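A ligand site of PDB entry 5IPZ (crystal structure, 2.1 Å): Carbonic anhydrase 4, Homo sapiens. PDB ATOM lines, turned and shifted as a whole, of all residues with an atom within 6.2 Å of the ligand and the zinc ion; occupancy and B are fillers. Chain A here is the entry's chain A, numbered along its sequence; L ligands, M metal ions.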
ATOM      1  N   TRP A   6       0.168  -7.965 -29.368  1.00  0.00           N
ATOM      2  CA  TRP A   6      -0.830  -6.954 -29.699  1.00  0.00           C
ATOM      3  C   TRP A   6      -1.378  -6.394 -28.407  1.00  0.00           C
ATOM      4  O   TRP A   6      -1.256  -7.011 -27.358  1.00  0.00           O
ATOM      5  CB  TRP A   6      -1.935  -7.506 -30.539  1.00  0.00           C
ATOM      6  CG  TRP A   6      -2.686  -8.670 -29.902  1.00  0.00           C
ATOM      7  CD1 TRP A   6      -2.409 -10.036 -30.013  1.00  0.00           C
ATOM      8  CD2 TRP A   6      -3.872  -8.594 -29.021  1.00  0.00           C
ATOM      9  NE1 TRP A   6      -3.307 -10.782 -29.286  1.00  0.00           N
ATOM     10  CE2 TRP A   6      -4.217  -9.972 -28.664  1.00  0.00           C
ATOM     11  CE3 TRP A   6      -4.658  -7.553 -28.515  1.00  0.00           C
ATOM     12  CZ2 TRP A   6      -5.296 -10.272 -27.848  1.00  0.00           C
ATOM     13  CZ3 TRP A   6      -5.730  -7.873 -27.687  1.00  0.00           C
ATOM     14  CH2 TRP A   6      -6.052  -9.198 -27.365  1.00  0.00           C
ATOM     15  N   TYR A   8      -4.466  -3.328 -26.517  1.00  0.00           N
ATOM     16  CA  TYR A   8      -5.693  -2.507 -26.640  1.00  0.00           C
ATOM     17  C   TYR A   8      -5.234  -1.065 -26.599  1.00  0.00           C
ATOM     18  O   TYR A   8      -4.134  -0.787 -26.109  1.00  0.00           O
ATOM     19  CB  TYR A   8      -6.706  -2.801 -25.493  1.00  0.00           C
ATOM     20  CG  TYR A   8      -7.505  -4.080 -25.725  1.00  0.00           C
ATOM     21  CD1 TYR A   8      -8.413  -4.165 -26.783  1.00  0.00           C
ATOM     22  CD2 TYR A   8      -7.308  -5.225 -24.944  1.00  0.00           C
ATOM     23  CE1 TYR A   8      -9.128  -5.329 -27.038  1.00  0.00           C
ATOM     24  CE2 TYR A   8      -8.019  -6.410 -25.197  1.00  0.00           C
ATOM     25  CZ  TYR A   8      -8.922  -6.445 -26.257  1.00  0.00           C
ATOM     26  OH  TYR A   8      -9.649  -7.591 -26.533  1.00  0.00           O
ATOM     27  N   ASN A  69      -4.973 -14.133 -19.051  1.00  0.00           N
ATOM     28  CA  ASN A  69      -4.100 -14.340 -20.199  1.00  0.00           C
ATOM     29  C   ASN A  69      -3.450 -13.014 -20.613  1.00  0.00           C
ATOM     30  O   ASN A  69      -2.920 -12.907 -21.719  1.00  0.00           O
ATOM     31  CB  ASN A  69      -4.903 -14.894 -21.359  1.00  0.00           C
ATOM     32  CG  ASN A  69      -6.001 -13.945 -21.797  1.00  0.00           C
ATOM     33  OD1 ASN A  69      -6.075 -12.841 -21.264  1.00  0.00           O
ATOM     34  ND2 ASN A  69      -6.835 -14.335 -22.792  1.00  0.00           N
ATOM     35  N   HIS A  71      -5.056 -10.414 -21.525  1.00  0.00           N
ATOM     36  CA  HIS A  71      -6.006  -9.630 -22.326  1.00  0.00           C
ATOM     37  C   HIS A  71      -7.410  -9.606 -21.779  1.00  0.00           C
ATOM     38  O   HIS A  71      -8.178  -8.641 -22.002  1.00  0.00           O
ATOM     39  CB  HIS A  71      -6.060 -10.127 -23.741  1.00  0.00           C
ATOM     40  CG  HIS A  71      -4.741 -10.091 -24.453  1.00  0.00           C
ATOM     41  ND1 HIS A  71      -4.063  -8.949 -24.644  1.00  0.00           N
ATOM     42  CD2 HIS A  71      -4.002 -11.105 -25.044  1.00  0.00           C
ATOM     43  CE1 HIS A  71      -2.933  -9.223 -25.338  1.00  0.00           C
ATOM     44  NE2 HIS A  71      -2.910 -10.542 -25.590  1.00  0.00           N
ATOM     45  N   SER A  72      -7.761 -10.704 -21.101  1.00  0.00           N
ATOM     46  CA  SER A  72      -9.042 -10.845 -20.502  1.00  0.00           C
ATOM     47  C   SER A  72      -8.875 -11.816 -19.319  1.00  0.00           C
ATOM     48  O   SER A  72      -7.763 -12.264 -19.045  1.00  0.00           O
ATOM     49  CB  SER A  72      -9.972 -11.471 -21.511  1.00  0.00           C
ATOM     50  OG  SER A  72     -11.264 -11.438 -20.955  1.00  0.00           O
ATOM     51  N   MET A  74     -10.260 -15.655 -18.625  1.00  0.00           N
ATOM     52  CA  MET A  74     -10.867 -16.703 -19.446  1.00  0.00           C
ATOM     53  C   MET A  74     -11.079 -17.986 -18.651  1.00  0.00           C
ATOM     54  O   MET A  74     -10.151 -18.462 -17.975  1.00  0.00           O
ATOM     55  CB  MET A  74      -9.926 -17.034 -20.580  1.00  0.00           C
ATOM     56  CG  MET A  74     -10.488 -17.907 -21.670  1.00  0.00           C
ATOM     57  SD  MET A  74      -9.209 -18.229 -22.914  1.00  0.00           S
ATOM     58  CE  MET A  74      -9.848 -17.297 -24.278  1.00  0.00           C
ATOM     59  N   GLN A  96     -14.481 -21.821 -24.388  1.00  0.00           N
ATOM     60  CA  GLN A  96     -14.019 -20.897 -23.372  1.00  0.00           C
ATOM     61  C   GLN A  96     -15.058 -19.743 -23.184  1.00  0.00           C
ATOM     62  O   GLN A  96     -15.975 -19.614 -23.973  1.00  0.00           O
ATOM     63  CB  GLN A  96     -12.593 -20.409 -23.709  1.00  0.00           C
ATOM     64  CG  GLN A  96     -12.420 -19.933 -25.147  1.00  0.00           C
ATOM     65  CD  GLN A  96     -12.459 -18.408 -25.242  1.00  0.00           C
ATOM     66  OE1 GLN A  96     -12.960 -17.729 -24.334  1.00  0.00           O
ATOM     67  NE2 GLN A  96     -11.936 -17.856 -26.350  1.00  0.00           N
ATOM     68  N   HIS A  98     -15.041 -15.643 -21.699  1.00  0.00           N
ATOM     69  CA  HIS A  98     -14.242 -14.531 -21.247  1.00  0.00           C
ATOM     70  C   HIS A  98     -15.066 -13.276 -21.296  1.00  0.00           C
ATOM     71  O   HIS A  98     -16.180 -13.289 -21.802  1.00  0.00           O
ATOM     72  CB  HIS A  98     -13.005 -14.381 -22.169  1.00  0.00           C
ATOM     73  CG  HIS A  98     -13.328 -13.990 -23.604  1.00  0.00           C
ATOM     74  ND1 HIS A  98     -13.419 -14.888 -24.579  1.00  0.00           N
ATOM     75  CD2 HIS A  98     -13.554 -12.742 -24.196  1.00  0.00           C
ATOM     76  CE1 HIS A  98     -13.722 -14.288 -25.748  1.00  0.00           C
ATOM     77  NE2 HIS A  98     -13.747 -12.953 -25.544  1.00  0.00           N
ATOM     78  N   LEU A  99     -14.516 -12.158 -20.795  1.00  0.00           N
ATOM     79  CA  LEU A  99     -15.289 -10.952 -20.654  1.00  0.00           C
ATOM     80  C   LEU A  99     -14.510  -9.766 -21.207  1.00  0.00           C
ATOM     81  O   LEU A  99     -13.314  -9.866 -21.376  1.00  0.00           O
ATOM     82  CB  LEU A  99     -15.676 -10.710 -19.204  1.00  0.00           C
ATOM     83  CG  LEU A  99     -16.547 -11.798 -18.543  1.00  0.00           C
ATOM     84  CD1 LEU A  99     -15.621 -12.704 -17.738  1.00  0.00           C
ATOM     85  CD2 LEU A  99     -17.637 -11.211 -17.675  1.00  0.00           C
ATOM     86  N   HIS A 100     -15.208  -8.657 -21.487  1.00  0.00           N
ATOM     87  CA  HIS A 100     -14.528  -7.364 -21.747  1.00  0.00           C
ATOM     88  C   HIS A 100     -15.171  -6.394 -20.853  1.00  0.00           C
ATOM     89  O   HIS A 100     -16.380  -6.521 -20.628  1.00  0.00           O
ATOM     90  CB  HIS A 100     -14.732  -6.965 -23.223  1.00  0.00           C
ATOM     91  CG  HIS A 100     -14.294  -8.055 -24.192  1.00  0.00           C
ATOM     92  ND1 HIS A 100     -13.068  -8.083 -24.737  1.00  0.00           N
ATOM     93  CD2 HIS A 100     -14.969  -9.143 -24.703  1.00  0.00           C
ATOM     94  CE1 HIS A 100     -12.947  -9.116 -25.540  1.00  0.00           C
ATOM     95  NE2 HIS A 100     -14.116  -9.788 -25.527  1.00  0.00           N
ATOM     96  N   GLU A 110     -18.364  -4.381 -26.049  1.00  0.00           N
ATOM     97  CA  GLU A 110     -17.808  -4.338 -27.408  1.00  0.00           C
ATOM     98  C   GLU A 110     -18.914  -4.128 -28.393  1.00  0.00           C
ATOM     99  O   GLU A 110     -18.793  -3.300 -29.339  1.00  0.00           O
ATOM    100  CB  GLU A 110     -17.074  -5.627 -27.775  1.00  0.00           C
ATOM    101  CG  GLU A 110     -15.844  -5.886 -26.926  1.00  0.00           C
ATOM    102  CD  GLU A 110     -14.774  -6.725 -27.671  1.00  0.00           C
ATOM    103  OE1 GLU A 110     -15.044  -7.853 -28.098  1.00  0.00           O
ATOM    104  OE2 GLU A 110     -13.648  -6.221 -27.796  1.00  0.00           O
ATOM    105  N   GLU A 121     -18.930  -6.935 -21.339  1.00  0.00           N
ATOM    106  CA  GLU A 121     -19.561  -7.912 -22.186  1.00  0.00           C
ATOM    107  C   GLU A 121     -18.903  -9.296 -22.124  1.00  0.00           C
ATOM    108  O   GLU A 121     -17.728  -9.440 -22.329  1.00  0.00           O
ATOM    109  CB  GLU A 121     -19.681  -7.362 -23.589  1.00  0.00           C
ATOM    110  CG  GLU A 121     -20.179  -8.342 -24.632  1.00  0.00           C
ATOM    111  CD  GLU A 121     -20.137  -7.738 -26.028  1.00  0.00           C
ATOM    112  OE1 GLU A 121     -20.155  -6.508 -26.128  1.00  0.00           O
ATOM    113  OE2 GLU A 121     -20.077  -8.491 -27.045  1.00  0.00           O
ATOM    114  N   HIS A 123     -18.499 -13.204 -23.388  1.00  0.00           N
ATOM    115  CA  HIS A 123     -18.414 -14.068 -24.543  1.00  0.00           C
ATOM    116  C   HIS A 123     -18.235 -15.528 -24.237  1.00  0.00           C
ATOM    117  O   HIS A 123     -17.229 -15.947 -23.637  1.00  0.00           O
ATOM    118  CB  HIS A 123     -17.235 -13.624 -25.454  1.00  0.00           C
ATOM    119  CG  HIS A 123     -17.404 -12.246 -26.036  1.00  0.00           C
ATOM    120  ND1 HIS A 123     -16.394 -11.515 -26.530  1.00  0.00           N
ATOM    121  CD2 HIS A 123     -18.566 -11.494 -26.236  1.00  0.00           C
ATOM    122  CE1 HIS A 123     -16.878 -10.324 -26.986  1.00  0.00           C
ATOM    123  NE2 HIS A 123     -18.203 -10.330 -26.808  1.00  0.00           N
ATOM    124  N   ILE A 124     -19.168 -16.335 -24.675  1.00  0.00           N
ATOM    125  CA  ILE A 124     -19.002 -17.782 -24.560  1.00  0.00           C
ATOM    126  C   ILE A 124     -18.820 -18.299 -25.956  1.00  0.00           C
ATOM    127  O   ILE A 124     -19.744 -18.186 -26.750  1.00  0.00           O
ATOM    128  CB  ILE A 124     -20.204 -18.467 -23.848  1.00  0.00           C
ATOM    129  CG1 ILE A 124     -20.681 -17.591 -22.663  1.00  0.00           C
ATOM    130  CG2 ILE A 124     -19.808 -19.899 -23.420  1.00  0.00           C
ATOM    131  CD1 ILE A 124     -21.933 -18.109 -21.915  1.00  0.00           C
ATOM    132  N   VAL A 125     -17.598 -18.810 -26.221  1.00  0.00           N
ATOM    133  CA  VAL A 125     -17.032 -19.166 -27.543  1.00  0.00           C
ATOM    134  C   VAL A 125     -17.258 -20.696 -27.722  1.00  0.00           C
ATOM    135  O   VAL A 125     -16.828 -21.490 -26.876  1.00  0.00           O
ATOM    136  CB  VAL A 125     -15.478 -18.758 -27.608  1.00  0.00           C
ATOM    137  CG1 VAL A 125     -14.799 -19.214 -28.888  1.00  0.00           C
ATOM    138  CG2 VAL A 125     -15.268 -17.232 -27.478  1.00  0.00           C
ATOM    139  N   ILE A 146     -17.105 -20.836 -35.754  1.00  0.00           N
ATOM    140  CA  ILE A 146     -17.199 -20.490 -34.343  1.00  0.00           C
ATOM    141  C   ILE A 146     -18.516 -19.818 -34.030  1.00  0.00           C
ATOM    142  O   ILE A 146     -19.000 -19.051 -34.841  1.00  0.00           O
ATOM    143  CB  ILE A 146     -15.992 -19.645 -33.873  1.00  0.00           C
ATOM    144  CG1 ILE A 146     -14.822 -20.584 -33.544  1.00  0.00           C
ATOM    145  CG2 ILE A 146     -16.334 -18.820 -32.643  1.00  0.00           C
ATOM    146  CD1 ILE A 146     -13.578 -19.847 -33.070  1.00  0.00           C
ATOM    147  N   VAL A 148     -20.271 -17.507 -31.155  1.00  0.00           N
ATOM    148  CA  VAL A 148     -20.144 -16.770 -29.899  1.00  0.00           C
ATOM    149  C   VAL A 148     -21.510 -16.358 -29.331  1.00  0.00           C
ATOM    150  O   VAL A 148     -22.321 -15.784 -30.020  1.00  0.00           O
ATOM    151  CB  VAL A 148     -19.206 -15.537 -29.983  1.00  0.00           C
ATOM    152  CG1 VAL A 148     -19.155 -14.871 -28.626  1.00  0.00           C
ATOM    153  CG2 VAL A 148     -17.766 -15.962 -30.334  1.00  0.00           C
ATOM    154  N   SER A 206     -16.369 -11.627 -37.090  1.00  0.00           N
ATOM    155  CA  SER A 206     -14.993 -12.065 -36.806  1.00  0.00           C
ATOM    156  C   SER A 206     -14.768 -12.193 -35.309  1.00  0.00           C
ATOM    157  O   SER A 206     -15.649 -11.820 -34.537  1.00  0.00           O
ATOM    158  CB  SER A 206     -13.933 -11.103 -37.401  1.00  0.00           C
ATOM    159  OG  SER A 206     -13.800  -9.920 -36.625  1.00  0.00           O
ATOM    160  N   LEU A 207     -13.580 -12.638 -34.960  1.00  0.00           N
ATOM    161  CA  LEU A 207     -13.106 -12.693 -33.575  1.00  0.00           C
ATOM    162  C   LEU A 207     -12.790 -11.253 -33.355  1.00  0.00           C
ATOM    163  O   LEU A 207     -12.543 -10.568 -34.324  1.00  0.00           O
ATOM    164  CB  LEU A 207     -11.807 -13.479 -33.474  1.00  0.00           C
ATOM    165  CG  LEU A 207     -11.715 -15.001 -33.649  1.00  0.00           C
ATOM    166  CD1 LEU A 207     -10.440 -15.507 -32.987  1.00  0.00           C
ATOM    167  CD2 LEU A 207     -12.935 -15.694 -33.075  1.00  0.00           C
ATOM    168  N   THR A 208     -12.808 -10.772 -32.105  1.00  0.00           N
ATOM    169  CA  THR A 208     -12.642  -9.325 -31.934  1.00  0.00           C
ATOM    170  C   THR A 208     -11.244  -9.074 -31.445  1.00  0.00           C
ATOM    171  O   THR A 208     -10.934  -7.992 -31.005  1.00  0.00           O
ATOM    172  CB  THR A 208     -13.637  -8.692 -30.941  1.00  0.00           C
ATOM    173  OG1 THR A 208     -13.461  -9.256 -29.633  1.00  0.00           O
ATOM    174  CG2 THR A 208     -15.073  -8.863 -31.405  1.00  0.00           C
ATOM    175  N   THR A 209     -10.416 -10.116 -31.479  1.00  0.00           N
ATOM    176  CA  THR A 209      -9.000 -10.015 -31.139  1.00  0.00           C
ATOM    177  C   THR A 209      -8.206 -10.715 -32.230  1.00  0.00           C
ATOM    178  O   THR A 209      -8.791 -11.531 -32.987  1.00  0.00           O
ATOM    179  CB  THR A 209      -8.675 -10.713 -29.811  1.00  0.00           C
ATOM    180  OG1 THR A 209      -8.892 -12.106 -30.001  1.00  0.00           O
ATOM    181  CG2 THR A 209      -9.566 -10.159 -28.683  1.00  0.00           C
ATOM    182  N   VAL A 216     -17.013 -16.146 -37.544  1.00  0.00           N
ATOM    183  CA  VAL A 216     -17.910 -16.158 -36.369  1.00  0.00           C
ATOM    184  C   VAL A 216     -19.352 -15.882 -36.732  1.00  0.00           C
ATOM    185  O   VAL A 216     -19.669 -14.853 -37.355  1.00  0.00           O
ATOM    186  CB  VAL A 216     -17.467 -15.156 -35.303  1.00  0.00           C
ATOM    187  CG1 VAL A 216     -18.307 -15.295 -34.050  1.00  0.00           C
ATOM    188  CG2 VAL A 216     -16.009 -15.375 -34.938  1.00  0.00           C
ATOM    189  N   TRP A 218     -22.454 -14.665 -35.015  1.00  0.00           N
ATOM    190  CA  TRP A 218     -22.635 -13.918 -33.773  1.00  0.00           C
ATOM    191  C   TRP A 218     -24.025 -13.982 -33.214  1.00  0.00           C
ATOM    192  O   TRP A 218     -24.977 -14.007 -33.986  1.00  0.00           O
ATOM    193  CB  TRP A 218     -22.230 -12.451 -33.950  1.00  0.00           C
ATOM    194  CG  TRP A 218     -20.747 -12.250 -33.818  1.00  0.00           C
ATOM    195  CD1 TRP A 218     -19.797 -12.198 -34.833  1.00  0.00           C
ATOM    196  CD2 TRP A 218     -19.989 -12.112 -32.577  1.00  0.00           C
ATOM    197  NE1 TRP A 218     -18.547 -12.030 -34.318  1.00  0.00           N
ATOM    198  CE2 TRP A 218     -18.585 -11.963 -32.967  1.00  0.00           C
ATOM    199  CE3 TRP A 218     -20.319 -12.085 -31.225  1.00  0.00           C
ATOM    200  CZ2 TRP A 218     -17.585 -11.808 -32.030  1.00  0.00           C
ATOM    201  CZ3 TRP A 218     -19.295 -11.926 -30.290  1.00  0.00           C
ATOM    202  CH2 TRP A 218     -17.961 -11.795 -30.697  1.00  0.00           C
HETATM  203  C1  LIG L   1      -9.113 -13.174 -26.649  1.00  0.00           C
HETATM  204 CL1  LIG L   1     -14.346 -15.925 -30.640  1.00  0.00          CL
HETATM  205  C2  LIG L   1     -12.902 -15.521 -29.657  1.00  0.00           C
HETATM  206  C3  LIG L   1     -12.739 -14.280 -29.025  1.00  0.00           C
HETATM  207  S1  LIG L   1     -14.036 -13.074 -29.162  1.00  0.00           S
HETATM  208  O1  LIG L   1     -15.353 -13.752 -28.633  1.00  0.00           O
HETATM  209  O2  LIG L   1     -14.371 -12.828 -30.639  1.00  0.00           O
HETATM  210  N1  LIG L   1     -13.749 -11.640 -28.292  1.00  0.00           N
HETATM  211  C4  LIG L   1     -11.597 -13.911 -28.256  1.00  0.00           C
HETATM  212  C5  LIG L   1     -11.810 -16.419 -29.504  1.00  0.00           C
HETATM  213  C6  LIG L   1     -10.663 -16.058 -28.735  1.00  0.00           C
HETATM  214  C7  LIG L   1     -10.535 -14.804 -28.099  1.00  0.00           C
HETATM  215  C8  LIG L   1      -9.331 -14.426 -27.272  1.00  0.00           C
HETATM  216  N2  LIG L   1      -8.321 -15.337 -27.027  1.00  0.00           N
HETATM  217  C9  LIG L   1      -7.321 -14.819 -26.273  1.00  0.00           C
HETATM  218  N3  LIG L   1      -6.194 -15.586 -25.913  1.00  0.00           N
HETATM  219  S2  LIG L   1      -7.654 -13.262 -25.842  1.00  0.00           S
HETATM  220 ZN    ZN M   1     -14.473 -11.514 -26.514  1.00  0.00          ZN
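The side-chain amide oxygen (OE1) of Gln 96 lies within hydrogen-bond range of a ring nitrogen (ND1) of His 98, at 2.9 Å. The side-chain carboxylate (OE2) of Glu 121 is in hydrogen-bond range of a ring nitrogen (NE2) of His 123. NE2 of His 100 lies close to OE1 of Glu 110 (3.3 Å). The side-chain carboxylate (OE1) of Glu 110 sits at hydrogen-bond distance from the side-chain hydroxyl (OG1) of Thr 208, 2.6 Å away. The backbone carbonyl oxygen (O) of Gln 96 sits at hydrogen-bond distance from the backbone NH (N) of Val 125, at 2.9 Å. The backbone NH (N) of His 71 sits at hydrogen-bond distance from the side-chain amide oxygen (OD1) of Asn 69 (2.6 Å). N of Ser 72 is in hydrogen-bond range of OD1 of Asn 69, at 2.7 Å. NE1 of Trp 218 sits at hydrogen-bond distance from O of Ser 206.
OG1 of Thr 208 touches the zinc ion, 3.98 Å away. Within 4 Å of the zinc ion: His 98, His 100, His 123 and Thr 208.
CE of Met 74 touches N2 of the ligand, at 3.7 Å. Gln 96 touches the ligand (NE2 to C6, 3.2 Å). Val 125 touches the ligand. Val 148 touches the ligand (CG2 to CL1, 3.4 Å). Leu 207 touches the ligand. Thr 209 touches the ligand (OG1 to C1, 3.5 Å). CZ2 of Trp 218 touches O2 of the ligand, at 3.6 Å. 12 residues have an atom within 4 Å of the ligand: Asn 69, Met 74, Gln 96, His 98, His 100, His 123, Val 125, Val 148, Leu 207, Thr 208, Thr 209 and Trp 218.
The backbone NH of Thr 208 is in hydrogen-bond range of an oxygen (O2) of the ligand. The side-chain hydroxyl (OG1) of Thr 208 sits close to a nitrogen (N1) of the ligand. A sulfur (S2) of the ligand lies close to the side-chain amide nitrogen (ND2) of Asn 69.
The zinc ion is bound by NE2 of His 98 (1.9 Å), ND1 of His 123 (1.9 Å), N1 of the ligand (1.9 Å) and NE2 of His 100 (2.0 Å).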
